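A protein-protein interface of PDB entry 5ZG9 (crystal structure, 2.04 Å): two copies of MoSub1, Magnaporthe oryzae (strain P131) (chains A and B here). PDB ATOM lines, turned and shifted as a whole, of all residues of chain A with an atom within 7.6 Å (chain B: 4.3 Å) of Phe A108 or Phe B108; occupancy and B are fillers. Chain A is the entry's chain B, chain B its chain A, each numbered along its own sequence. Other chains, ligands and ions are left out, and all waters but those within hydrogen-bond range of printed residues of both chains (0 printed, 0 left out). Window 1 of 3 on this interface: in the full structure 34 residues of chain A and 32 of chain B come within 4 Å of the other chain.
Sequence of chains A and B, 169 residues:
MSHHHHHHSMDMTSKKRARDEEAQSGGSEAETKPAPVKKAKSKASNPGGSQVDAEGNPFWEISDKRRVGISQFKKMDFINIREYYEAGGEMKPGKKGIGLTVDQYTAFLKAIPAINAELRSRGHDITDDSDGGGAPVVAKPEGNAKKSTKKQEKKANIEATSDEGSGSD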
ATOM      1  N   TRP A  60      15.502  15.175  15.460  1.00  0.00           N
ATOM      2  CA  TRP A  60      16.054  16.198  14.565  1.00  0.00           C
ATOM      3  C   TRP A  60      14.908  17.135  14.176  1.00  0.00           C
ATOM      4  O   TRP A  60      13.822  16.671  13.817  1.00  0.00           O
ATOM      5  CB  TRP A  60      16.607  15.524  13.301  1.00  0.00           C
ATOM      6  CG  TRP A  60      17.784  14.647  13.604  1.00  0.00           C
ATOM      7  CD1 TRP A  60      19.116  15.001  13.580  1.00  0.00           C
ATOM      8  CD2 TRP A  60      17.735  13.282  14.040  1.00  0.00           C
ATOM      9  NE1 TRP A  60      19.886  13.919  13.949  1.00  0.00           N
ATOM     10  CE2 TRP A  60      19.069  12.859  14.240  1.00  0.00           C
ATOM     11  CE3 TRP A  60      16.700  12.379  14.268  1.00  0.00           C
ATOM     12  CZ2 TRP A  60      19.382  11.556  14.652  1.00  0.00           C
ATOM     13  CZ3 TRP A  60      17.009  11.094  14.677  1.00  0.00           C
ATOM     14  CH2 TRP A  60      18.345  10.694  14.870  1.00  0.00           C
ATOM     15  N   GLU A  61      15.113  18.439  14.261  1.00  0.00           N
ATOM     16  CA  GLU A  61      14.024  19.376  13.986  1.00  0.00           C
ATOM     17  C   GLU A  61      13.886  19.542  12.487  1.00  0.00           C
ATOM     18  O   GLU A  61      14.888  19.623  11.773  1.00  0.00           O
ATOM     19  CB  GLU A  61      14.302  20.727  14.630  1.00  0.00           C
ATOM     20  CG  GLU A  61      14.261  20.684  16.147  1.00  0.00           C
ATOM     21  CD  GLU A  61      14.762  21.968  16.778  1.00  0.00           C
ATOM     22  OE1 GLU A  61      15.048  22.933  16.033  1.00  0.00           O
ATOM     23  OE2 GLU A  61      14.872  22.007  18.022  1.00  0.00           O
ATOM     24  N   ILE A  62      12.653  19.572  12.002  1.00  0.00           N
ATOM     25  CA  ILE A  62      12.443  19.825  10.583  1.00  0.00           C
ATOM     26  C   ILE A  62      11.579  21.064  10.400  1.00  0.00           C
ATOM     27  O   ILE A  62      11.285  21.481   9.270  1.00  0.00           O
ATOM     28  CB  ILE A  62      11.837  18.619   9.866  1.00  0.00           C
ATOM     29  CG1 ILE A  62      10.475  18.265  10.455  1.00  0.00           C
ATOM     30  CG2 ILE A  62      12.789  17.419   9.955  1.00  0.00           C
ATOM     31  CD1 ILE A  62       9.796  17.122   9.712  1.00  0.00           C
ATOM     32  N   SER A  63      11.168  21.633  11.533  1.00  0.00           N
ATOM     33  CA  SER A  63      10.523  22.939  11.581  1.00  0.00           C
ATOM     34  C   SER A  63      10.442  23.365  13.043  1.00  0.00           C
ATOM     35  O   SER A  63      10.949  22.665  13.932  1.00  0.00           O
ATOM     36  CB  SER A  63       9.129  22.901  10.955  1.00  0.00           C
ATOM     37  OG  SER A  63       8.143  22.480  11.884  1.00  0.00           O
ATOM     38  N   ARG A  67       9.161  17.412  14.368  1.00  0.00           N
ATOM     39  CA  ARG A  67      10.354  16.590  14.585  1.00  0.00           C
ATOM     40  C   ARG A  67      10.255  15.255  13.858  1.00  0.00           C
ATOM     41  O   ARG A  67       9.155  14.741  13.604  1.00  0.00           O
ATOM     42  CB  ARG A  67      10.534  16.280  16.076  1.00  0.00           C
ATOM     43  CG  ARG A  67      10.745  17.475  17.005  1.00  0.00           C
ATOM     44  CD  ARG A  67      10.638  17.025  18.467  1.00  0.00           C
ATOM     45  NE  ARG A  67      10.659  18.160  19.383  1.00  0.00           N
ATOM     46  CZ  ARG A  67      10.847  18.069  20.694  1.00  0.00           C
ATOM     47  NH1 ARG A  67      11.054  16.886  21.259  1.00  0.00           N
ATOM     48  NH2 ARG A  67      10.851  19.165  21.432  1.00  0.00           N
ATOM     49  N   VAL A  68      11.404  14.689  13.522  1.00  0.00           N
ATOM     50  CA  VAL A  68      11.453  13.282  13.146  1.00  0.00           C
ATOM     51  C   VAL A  68      12.277  12.573  14.227  1.00  0.00           C
ATOM     52  O   VAL A  68      13.433  12.957  14.491  1.00  0.00           O
ATOM     53  CB  VAL A  68      12.046  13.063  11.730  1.00  0.00           C
ATOM     54  CG1 VAL A  68      13.293  13.843  11.537  1.00  0.00           C
ATOM     55  CG2 VAL A  68      12.309  11.569  11.474  1.00  0.00           C
ATOM     56  N   GLY A  69      11.694  11.610  14.922  1.00  0.00           N
ATOM     57  CA  GLY A  69      12.438  11.015  16.029  1.00  0.00           C
ATOM     58  C   GLY A  69      12.486   9.507  15.928  1.00  0.00           C
ATOM     59  O   GLY A  69      11.738   8.923  15.144  1.00  0.00           O
ATOM     60  N   ILE A  79      10.249   5.291  13.425  1.00  0.00           N
ATOM     61  CA  ILE A  79      10.680   6.621  13.004  1.00  0.00           C
ATOM     62  C   ILE A  79       9.444   7.496  12.909  1.00  0.00           C
ATOM     63  O   ILE A  79       8.662   7.362  11.965  1.00  0.00           O
ATOM     64  CB  ILE A  79      11.382   6.575  11.627  1.00  0.00           C
ATOM     65  CG1 ILE A  79      12.652   5.718  11.702  1.00  0.00           C
ATOM     66  CG2 ILE A  79      11.701   7.990  11.142  1.00  0.00           C
ATOM     67  CD1 ILE A  79      12.435   4.198  11.532  1.00  0.00           C
ATOM     68  N   ASN A  80       9.238   8.354  13.906  1.00  0.00           N
ATOM     69  CA  ASN A  80       8.070   9.227  13.937  1.00  0.00           C
ATOM     70  C   ASN A  80       8.381  10.603  13.361  1.00  0.00           C
ATOM     71  O   ASN A  80       9.360  11.251  13.753  1.00  0.00           O
ATOM     72  CB  ASN A  80       7.575   9.417  15.378  1.00  0.00           C
ATOM     73  CG  ASN A  80       6.599   8.342  15.806  1.00  0.00           C
ATOM     74  OD1 ASN A  80       5.370   8.481  15.636  1.00  0.00           O
ATOM     75  ND2 ASN A  80       7.131   7.254  16.361  1.00  0.00           N
ATOM     76  N   ILE A  81       7.534  11.044  12.441  1.00  0.00           N
ATOM     77  CA  ILE A  81       7.607  12.383  11.851  1.00  0.00           C
ATOM     78  C   ILE A  81       6.318  13.030  12.318  1.00  0.00           C
ATOM     79  O   ILE A  81       5.227  12.624  11.887  1.00  0.00           O
ATOM     80  CB  ILE A  81       7.569  12.286  10.326  1.00  0.00           C
ATOM     81  CG1 ILE A  81       8.665  11.319   9.849  1.00  0.00           C
ATOM     82  CG2 ILE A  81       7.730  13.667   9.692  1.00  0.00           C
ATOM     83  CD1 ILE A  81       8.467  10.791   8.434  1.00  0.00           C
ATOM     84  N   LEU A 100       6.672   5.367  11.348  1.00  0.00           N
ATOM     85  CA  LEU A 100       7.063   4.377  10.353  1.00  0.00           C
ATOM     86  C   LEU A 100       7.855   3.252  11.005  1.00  0.00           C
ATOM     87  O   LEU A 100       8.714   3.503  11.861  1.00  0.00           O
ATOM     88  CB  LEU A 100       7.954   5.040   9.308  1.00  0.00           C
ATOM     89  CG  LEU A 100       7.368   6.319   8.700  1.00  0.00           C
ATOM     90  CD1 LEU A 100       8.362   6.954   7.724  1.00  0.00           C
ATOM     91  CD2 LEU A 100       6.041   5.982   7.991  1.00  0.00           C
ATOM     92  N   VAL A 102      10.802   0.367  10.477  1.00  0.00           N
ATOM     93  CA  VAL A 102      12.065   0.502   9.769  1.00  0.00           C
ATOM     94  C   VAL A 102      11.894   0.127   8.286  1.00  0.00           C
ATOM     95  O   VAL A 102      12.358   0.850   7.397  1.00  0.00           O
ATOM     96  CB  VAL A 102      13.166  -0.329  10.437  1.00  0.00           C
ATOM     97  CG1 VAL A 102      14.461  -0.278   9.617  1.00  0.00           C
ATOM     98  CG2 VAL A 102      13.403   0.191  11.853  1.00  0.00           C
ATOM     99  N   ASP A 103      11.212  -0.982   8.020  1.00  0.00           N
ATOM    100  CA  ASP A 103      10.915  -1.362   6.637  1.00  0.00           C
ATOM    101  C   ASP A 103      10.219  -0.224   5.872  1.00  0.00           C
ATOM    102  O   ASP A 103      10.575   0.063   4.722  1.00  0.00           O
ATOM    103  CB  ASP A 103      10.083  -2.649   6.586  1.00  0.00           C
ATOM    104  CG  ASP A 103      10.894  -3.888   6.966  1.00  0.00           C
ATOM    105  OD1 ASP A 103      12.143  -3.798   7.062  1.00  0.00           O
ATOM    106  OD2 ASP A 103      10.285  -4.963   7.155  1.00  0.00           O
ATOM    107  N   GLN A 104       9.262   0.451   6.508  1.00  0.00           N
ATOM    108  CA  GLN A 104       8.565   1.551   5.836  1.00  0.00           C
ATOM    109  C   GLN A 104       9.508   2.732   5.614  1.00  0.00           C
ATOM    110  O   GLN A 104       9.449   3.411   4.587  1.00  0.00           O
ATOM    111  CB  GLN A 104       7.306   1.979   6.612  1.00  0.00           C
ATOM    112  CG  GLN A 104       6.199   0.905   6.616  1.00  0.00           C
ATOM    113  CD  GLN A 104       5.134   1.172   7.689  1.00  0.00           C
ATOM    114  OE1 GLN A 104       5.170   2.196   8.389  1.00  0.00           O
ATOM    115  NE2 GLN A 104       4.181   0.257   7.811  1.00  0.00           N
ATOM    116  N   TYR A 105      10.377   2.987   6.580  1.00  0.00           N
ATOM    117  CA  TYR A 105      11.341   4.060   6.421  1.00  0.00           C
ATOM    118  C   TYR A 105      12.250   3.776   5.213  1.00  0.00           C
ATOM    119  O   TYR A 105      12.468   4.653   4.370  1.00  0.00           O
ATOM    120  CB  TYR A 105      12.148   4.247   7.713  1.00  0.00           C
ATOM    121  CG  TYR A 105      13.285   5.221   7.599  1.00  0.00           C
ATOM    122  CD1 TYR A 105      13.044   6.585   7.456  1.00  0.00           C
ATOM    123  CD2 TYR A 105      14.598   4.783   7.650  1.00  0.00           C
ATOM    124  CE1 TYR A 105      14.095   7.489   7.362  1.00  0.00           C
ATOM    125  CE2 TYR A 105      15.655   5.674   7.552  1.00  0.00           C
ATOM    126  CZ  TYR A 105      15.392   7.023   7.404  1.00  0.00           C
ATOM    127  OH  TYR A 105      16.432   7.906   7.307  1.00  0.00           O
ATOM    128  N   THR A 106      12.745   2.547   5.103  1.00  0.00           N
ATOM    129  CA  THR A 106      13.639   2.208   4.000  1.00  0.00           C
ATOM    130  C   THR A 106      12.905   2.269   2.654  1.00  0.00           C
ATOM    131  O   THR A 106      13.483   2.649   1.627  1.00  0.00           O
ATOM    132  CB  THR A 106      14.333   0.826   4.194  1.00  0.00           C
ATOM    133  OG1 THR A 106      13.360  -0.222   4.200  1.00  0.00           O
ATOM    134  CG2 THR A 106      15.095   0.792   5.504  1.00  0.00           C
ATOM    135  N   ALA A 107      11.630   1.901   2.655  1.00  0.00           N
ATOM    136  CA  ALA A 107      10.835   2.036   1.431  1.00  0.00           C
ATOM    137  C   ALA A 107      10.768   3.516   1.015  1.00  0.00           C
ATOM    138  O   ALA A 107      10.874   3.855  -0.166  1.00  0.00           O
ATOM    139  CB  ALA A 107       9.442   1.463   1.623  1.00  0.00           C
ATOM    140  N   PHE A 108      10.613   4.389   2.000  1.00  0.00           N
ATOM    141  CA  PHE A 108      10.588   5.822   1.767  1.00  0.00           C
ATOM    142  C   PHE A 108      11.946   6.281   1.228  1.00  0.00           C
ATOM    143  O   PHE A 108      12.015   7.133   0.340  1.00  0.00           O
ATOM    144  CB  PHE A 108      10.274   6.529   3.086  1.00  0.00           C
ATOM    145  CG  PHE A 108      10.371   8.018   3.022  1.00  0.00           C
ATOM    146  CD1 PHE A 108       9.429   8.762   2.333  1.00  0.00           C
ATOM    147  CD2 PHE A 108      11.396   8.682   3.668  1.00  0.00           C
ATOM    148  CE1 PHE A 108       9.509  10.148   2.293  1.00  0.00           C
ATOM    149  CE2 PHE A 108      11.487  10.063   3.610  1.00  0.00           C
ATOM    150  CZ  PHE A 108      10.533  10.794   2.934  1.00  0.00           C
ATOM    151  N   LEU A 109      13.023   5.719   1.775  1.00  0.00           N
ATOM    152  CA  LEU A 109      14.372   6.021   1.285  1.00  0.00           C
ATOM    153  C   LEU A 109      14.485   5.714  -0.206  1.00  0.00           C
ATOM    154  O   LEU A 109      15.049   6.502  -0.965  1.00  0.00           O
ATOM    155  CB  LEU A 109      15.429   5.217   2.056  1.00  0.00           C
ATOM    156  CG  LEU A 109      16.234   5.964   3.124  1.00  0.00           C
ATOM    157  CD1 LEU A 109      15.372   6.974   3.836  1.00  0.00           C
ATOM    158  CD2 LEU A 109      16.882   5.005   4.126  1.00  0.00           C
ATOM    159  N   LYS A 110      13.929   4.584  -0.623  1.00  0.00           N
ATOM    160  CA  LYS A 110      14.009   4.181  -2.024  1.00  0.00           C
ATOM    161  C   LYS A 110      13.263   5.135  -2.968  1.00  0.00           C
ATOM    162  O   LYS A 110      13.690   5.345  -4.100  1.00  0.00           O
ATOM    163  CB  LYS A 110      13.533   2.738  -2.200  1.00  0.00           C
ATOM    164  CG  LYS A 110      13.689   2.228  -3.616  1.00  0.00           C
ATOM    165  CD  LYS A 110      13.349   0.752  -3.727  1.00  0.00           C
ATOM    166  CE  LYS A 110      14.434  -0.113  -3.112  1.00  0.00           C
ATOM    167  NZ  LYS A 110      14.174  -1.560  -3.357  1.00  0.00           N
ATOM    168  N   ALA A 111      12.180   5.740  -2.478  1.00  0.00           N
ATOM    169  CA  ALA A 111      11.363   6.676  -3.262  1.00  0.00           C
ATOM    170  C   ALA A 111      11.940   8.096  -3.399  1.00  0.00           C
ATOM    171  O   ALA A 111      11.512   8.879  -4.250  1.00  0.00           O
ATOM    172  CB  ALA A 111       9.935   6.746  -2.672  1.00  0.00           C
ATOM    173  N   ILE A 112      12.894   8.434  -2.542  1.00  0.00           N
ATOM    174  CA  ILE A 112      13.456   9.780  -2.529  1.00  0.00           C
ATOM    175  C   ILE A 112      13.941  10.330  -3.879  1.00  0.00           C
ATOM    176  O   ILE A 112      13.662  11.489  -4.194  1.00  0.00           O
ATOM    177  CB  ILE A 112      14.497   9.929  -1.407  1.00  0.00           C
ATOM    178  CG1 ILE A 112      13.750  10.100  -0.088  1.00  0.00           C
ATOM    179  CG2 ILE A 112      15.441  11.116  -1.644  1.00  0.00           C
ATOM    180  CD1 ILE A 112      14.665  10.223   1.105  1.00  0.00           C
ATOM    181  N   PRO A 113      14.642   9.514  -4.692  1.00  0.00           N
ATOM    182  CA  PRO A 113      15.083  10.140  -5.944  1.00  0.00           C
ATOM    183  C   PRO A 113      13.890  10.524  -6.811  1.00  0.00           C
ATOM    184  O   PRO A 113      13.882  11.628  -7.364  1.00  0.00           O
ATOM    185  CB  PRO A 113      15.914   9.044  -6.616  1.00  0.00           C
ATOM    186  CG  PRO A 113      16.383   8.180  -5.487  1.00  0.00           C
ATOM    187  CD  PRO A 113      15.225   8.172  -4.517  1.00  0.00           C
ATOM    188  N   ILE A 115      10.783  11.205  -5.762  1.00  0.00           N
ATOM    189  CA  ILE A 115      10.166  12.360  -5.111  1.00  0.00           C
ATOM    190  C   ILE A 115      10.949  13.625  -5.453  1.00  0.00           C
ATOM    191  O   ILE A 115      10.367  14.664  -5.797  1.00  0.00           O
ATOM    192  CB  ILE A 115      10.138  12.201  -3.568  1.00  0.00           C
ATOM    193  CG1 ILE A 115       9.156  11.099  -3.171  1.00  0.00           C
ATOM    194  CG2 ILE A 115       9.730  13.505  -2.889  1.00  0.00           C
ATOM    195  CD1 ILE A 115       9.435  10.517  -1.802  1.00  0.00           C
ATOM    196  N   ILE B  62       4.717   2.700   0.597  1.00  0.00           N
ATOM    197  CA  ILE B  62       5.700   2.325   1.617  1.00  0.00           C
ATOM    198  C   ILE B  62       5.251   1.139   2.471  1.00  0.00           C
ATOM    199  O   ILE B  62       6.069   0.485   3.106  1.00  0.00           O
ATOM    200  CB  ILE B  62       6.135   3.507   2.467  1.00  0.00           C
ATOM    201  CG1 ILE B  62       4.948   4.105   3.221  1.00  0.00           C
ATOM    202  CG2 ILE B  62       6.801   4.559   1.590  1.00  0.00           C
ATOM    203  CD1 ILE B  62       5.378   4.939   4.422  1.00  0.00           C
ATOM    204  N   VAL B  68       3.660   7.579   0.237  1.00  0.00           N
ATOM    205  CA  VAL B  68       4.252   8.905   0.194  1.00  0.00           C
ATOM    206  C   VAL B  68       3.816   9.460  -1.151  1.00  0.00           C
ATOM    207  O   VAL B  68       3.831   8.740  -2.166  1.00  0.00           O
ATOM    208  CB  VAL B  68       5.783   8.854   0.241  1.00  0.00           C
ATOM    209  CG1 VAL B  68       6.356  10.275   0.328  1.00  0.00           C
ATOM    210  CG2 VAL B  68       6.226   8.075   1.448  1.00  0.00           C
ATOM    211  N   ILE B  81       2.913  11.899   3.764  1.00  0.00           N
ATOM    212  CA  ILE B  81       3.208  10.538   4.202  1.00  0.00           C
ATOM    213  C   ILE B  81       1.995  10.098   5.018  1.00  0.00           C
ATOM    214  O   ILE B  81       1.793  10.583   6.139  1.00  0.00           O
ATOM    215  CB  ILE B  81       4.486  10.511   5.087  1.00  0.00           C
ATOM    216  CG1 ILE B  81       5.637  11.216   4.363  1.00  0.00           C
ATOM    217  CG2 ILE B  81       4.872   9.074   5.482  1.00  0.00           C
ATOM    218  CD1 ILE B  81       6.897  11.404   5.197  1.00  0.00           C
ATOM    219  N   GLN B 104      10.261  21.643   4.917  1.00  0.00           N
ATOM    220  CA  GLN B 104      10.241  20.625   5.963  1.00  0.00           C
ATOM    221  C   GLN B 104      10.854  19.336   5.442  1.00  0.00           C
ATOM    222  O   GLN B 104      11.656  18.696   6.120  1.00  0.00           O
ATOM    223  CB  GLN B 104       8.817  20.399   6.450  1.00  0.00           C
ATOM    224  CG  GLN B 104       8.402  21.447   7.515  1.00  0.00           C
ATOM    225  CD  GLN B 104       6.895  21.520   7.709  1.00  0.00           C
ATOM    226  OE1 GLN B 104       6.180  20.592   7.351  1.00  0.00           O
ATOM    227  NE2 GLN B 104       6.408  22.633   8.271  1.00  0.00           N
ATOM    228  N   TYR B 105      10.475  18.975   4.222  1.00  0.00           N
ATOM    229  CA  TYR B 105      11.004  17.788   3.554  1.00  0.00           C
ATOM    230  C   TYR B 105      12.508  17.902   3.343  1.00  0.00           C
ATOM    231  O   TYR B 105      13.255  16.959   3.610  1.00  0.00           O
ATOM    232  CB  TYR B 105      10.292  17.603   2.217  1.00  0.00           C
ATOM    233  CG  TYR B 105      10.878  16.526   1.349  1.00  0.00           C
ATOM    234  CD1 TYR B 105      10.744  15.191   1.686  1.00  0.00           C
ATOM    235  CD2 TYR B 105      11.543  16.846   0.179  1.00  0.00           C
ATOM    236  CE1 TYR B 105      11.276  14.198   0.881  1.00  0.00           C
ATOM    237  CE2 TYR B 105      12.078  15.860  -0.637  1.00  0.00           C
ATOM    238  CZ  TYR B 105      11.948  14.540  -0.273  1.00  0.00           C
ATOM    239  OH  TYR B 105      12.473  13.549  -1.085  1.00  0.00           O
ATOM    240  N   THR B 106      12.951  19.063   2.874  1.00  0.00           N
ATOM    241  CA  THR B 106      14.377  19.323   2.701  1.00  0.00           C
ATOM    242  C   THR B 106      15.139  19.183   4.019  1.00  0.00           C
ATOM    243  O   THR B 106      16.241  18.628   4.043  1.00  0.00           O
ATOM    244  CB  THR B 106      14.628  20.720   2.115  1.00  0.00           C
ATOM    245  OG1 THR B 106      14.241  20.722   0.738  1.00  0.00           O
ATOM    246  CG2 THR B 106      16.094  21.083   2.213  1.00  0.00           C
ATOM    247  N   ALA B 107      14.554  19.680   5.110  1.00  0.00           N
ATOM    248  CA  ALA B 107      15.157  19.515   6.436  1.00  0.00           C
ATOM    249  C   ALA B 107      15.185  18.032   6.821  1.00  0.00           C
ATOM    250  O   ALA B 107      16.102  17.571   7.489  1.00  0.00           O
ATOM    251  CB  ALA B 107      14.389  20.313   7.475  1.00  0.00           C
ATOM    252  N   PHE B 108      14.170  17.285   6.399  1.00  0.00           N
ATOM    253  CA  PHE B 108      14.157  15.855   6.673  1.00  0.00           C
ATOM    254  C   PHE B 108      15.327  15.174   5.942  1.00  0.00           C
ATOM    255  O   PHE B 108      16.013  14.321   6.512  1.00  0.00           O
ATOM    256  CB  PHE B 108      12.810  15.246   6.291  1.00  0.00           C
ATOM    257  CG  PHE B 108      12.674  13.790   6.650  1.00  0.00           C
ATOM    258  CD1 PHE B 108      13.439  13.229   7.655  1.00  0.00           C
ATOM    259  CD2 PHE B 108      11.782  12.984   5.980  1.00  0.00           C
ATOM    260  CE1 PHE B 108      13.314  11.892   7.981  1.00  0.00           C
ATOM    261  CE2 PHE B 108      11.655  11.642   6.315  1.00  0.00           C
ATOM    262  CZ  PHE B 108      12.424  11.098   7.308  1.00  0.00           C
ATOM    263  N   LEU B 109      15.572  15.566   4.700  1.00  0.00           N
ATOM    264  CA  LEU B 109      16.660  14.964   3.933  1.00  0.00           C
ATOM    265  C   LEU B 109      18.005  15.174   4.629  1.00  0.00           C
ATOM    266  O   LEU B 109      18.857  14.284   4.630  1.00  0.00           O
ATOM    267  CB  LEU B 109      16.700  15.528   2.520  1.00  0.00           C
ATOM    268  CG  LEU B 109      15.470  15.170   1.681  1.00  0.00           C
ATOM    269  CD1 LEU B 109      15.634  15.559   0.219  1.00  0.00           C
ATOM    270  CD2 LEU B 109      15.199  13.693   1.810  1.00  0.00           C
ATOM    271  N   LYS B 110      18.161  16.339   5.253  1.00  0.00           N
ATOM    272  CA  LYS B 110      19.405  16.720   5.918  1.00  0.00           C
ATOM    273  C   LYS B 110      19.687  15.818   7.122  1.00  0.00           C
ATOM    274  O   LYS B 110      20.838  15.625   7.512  1.00  0.00           O
ATOM    275  CB  LYS B 110      19.314  18.185   6.353  1.00  0.00           C
ATOM    276  CG  LYS B 110      20.641  18.846   6.665  1.00  0.00           C
ATOM    277  CD  LYS B 110      20.465  20.349   6.864  1.00  0.00           C
ATOM    278  CE  LYS B 110      21.800  21.042   7.099  1.00  0.00           C
ATOM    279  NZ  LYS B 110      21.658  22.521   7.211  1.00  0.00           N
ATOM    280  N   ALA B 111      18.624  15.252   7.688  1.00  0.00           N
ATOM    281  CA  ALA B 111      18.715  14.439   8.899  1.00  0.00           C
ATOM    282  C   ALA B 111      18.979  12.967   8.594  1.00  0.00           C
ATOM    283  O   ALA B 111      19.425  12.216   9.461  1.00  0.00           O
ATOM    284  CB  ALA B 111      17.422  14.589   9.730  1.00  0.00           C
ATOM    285  N   ILE B 112      18.682  12.551   7.366  1.00  0.00           N
ATOM    286  CA  ILE B 112      18.755  11.139   6.999  1.00  0.00           C
ATOM    287  C   ILE B 112      20.050  10.405   7.370  1.00  0.00           C
ATOM    288  O   ILE B 112      19.981   9.325   7.971  1.00  0.00           O
ATOM    289  CB  ILE B 112      18.349  10.920   5.528  1.00  0.00           C
ATOM    290  CG1 ILE B 112      16.848  11.182   5.401  1.00  0.00           C
ATOM    291  CG2 ILE B 112      18.672   9.504   5.067  1.00  0.00           C
ATOM    292  CD1 ILE B 112      16.311  10.990   4.003  1.00  0.00           C
ATOM    293  N   ILE B 115      19.938   9.768  11.127  1.00  0.00           N
ATOM    294  CA  ILE B 115      18.886   8.790  11.377  1.00  0.00           C
ATOM    295  C   ILE B 115      19.375   7.382  11.025  1.00  0.00           C
ATOM    296  O   ILE B 115      19.200   6.429  11.804  1.00  0.00           O
ATOM    297  CB  ILE B 115      17.641   9.125  10.559  1.00  0.00           C
ATOM    298  CG1 ILE B 115      17.083  10.477  11.018  1.00  0.00           C
ATOM    299  CG2 ILE B 115      16.607   8.032  10.693  1.00  0.00           C
ATOM    300  CD1 ILE B 115      15.931  11.018  10.183  1.00  0.00           C
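Val A68 touches Phe B108, and with the chains exchanged Phe A108 touches Val B68. Ile B81 touches its own counterpart, Ile A81. Tyr A105 touches Ile B115, and with the chains exchanged Ile A115 touches Tyr B105. Ile B112 touches its own counterpart, Ile A112. Positions printed for both chains: 62, 68, 81, 104, 105, 106, 107, 108, 109, 110, 111, 112 and 115. Of the 24 pairs that touch across the chains among the printed residues, 17 have their exchanged pair printed and touching as well.
Ala B111 touches Trp A60 (CB to CB, 3.8 Å). Ile A62 touches Gln B104. CD2 of Leu A100 touches CD1 of Ile B62, at 3.8 Å. Ile B62 touches Gln A104. Phe B108 touches Tyr A105. Tyr A105 touches Ile B112. Tyr A105 touches Ile B115. Phe A108 touches Ile B62 (N to CG2, 3.8 Å). Phe B108 touches Phe A108. CD1 of Ile A115 touches CG1 of Val B68, 3.8 Å away.
Printed residues of chain B within 4 Å of Tyr A105: Phe B108, Ile B112 and Ile B115. Of the printed residues of chain B, Ile A115 touches Val B68 and Tyr B105. Of the printed residues of chain A, Gln B104 touches Ile A62 (3.4 Å) and Ser A63 (3.8 Å). Printed residues of chain A within 4 Å of Ala B107: Ile A62 (3.7 Å). Of the printed residues of chain A, Ile B112 touches Tyr A105 and Ile A112. The nearest residue of chain B that does not touch Phe A108 is Tyr B105 (4.04 Å). The nearest residue of chain A that does not touch Phe B108 is Ile A79 (5.0 Å). The nearest printed residue of chain B that does not touch Ile A115 is Leu B109 (7.0 Å).
Of the 24 printed residues of chain A, 12 touch a printed residue of chain B. Hydrophobic or aromatic side chains of chain A that line the printed part of chain B: Trp A60, Ile A62, Val A68, Ile A81, Leu A100, Tyr A105, Ala A107, Phe A108, Ile A112 and Ile A115. Along chain A the printed residues that touch a printed residue of chain B span positions 60 to 115. Among the printed residues, 24 pairs touch across the chains. Among the printed residues, no Asp or Glu carboxylate lies within 4 Å of a Lys or Arg side-chain nitrogen of the other chain.
The backbone NH (N) of Ile A79 is in hydrogen-bond range of the backbone carbonyl oxygen (O) of Leu A100, 2.8 Å away. O of Trp A60 is in hydrogen-bond range of N of Val A68 (3.1 Å).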
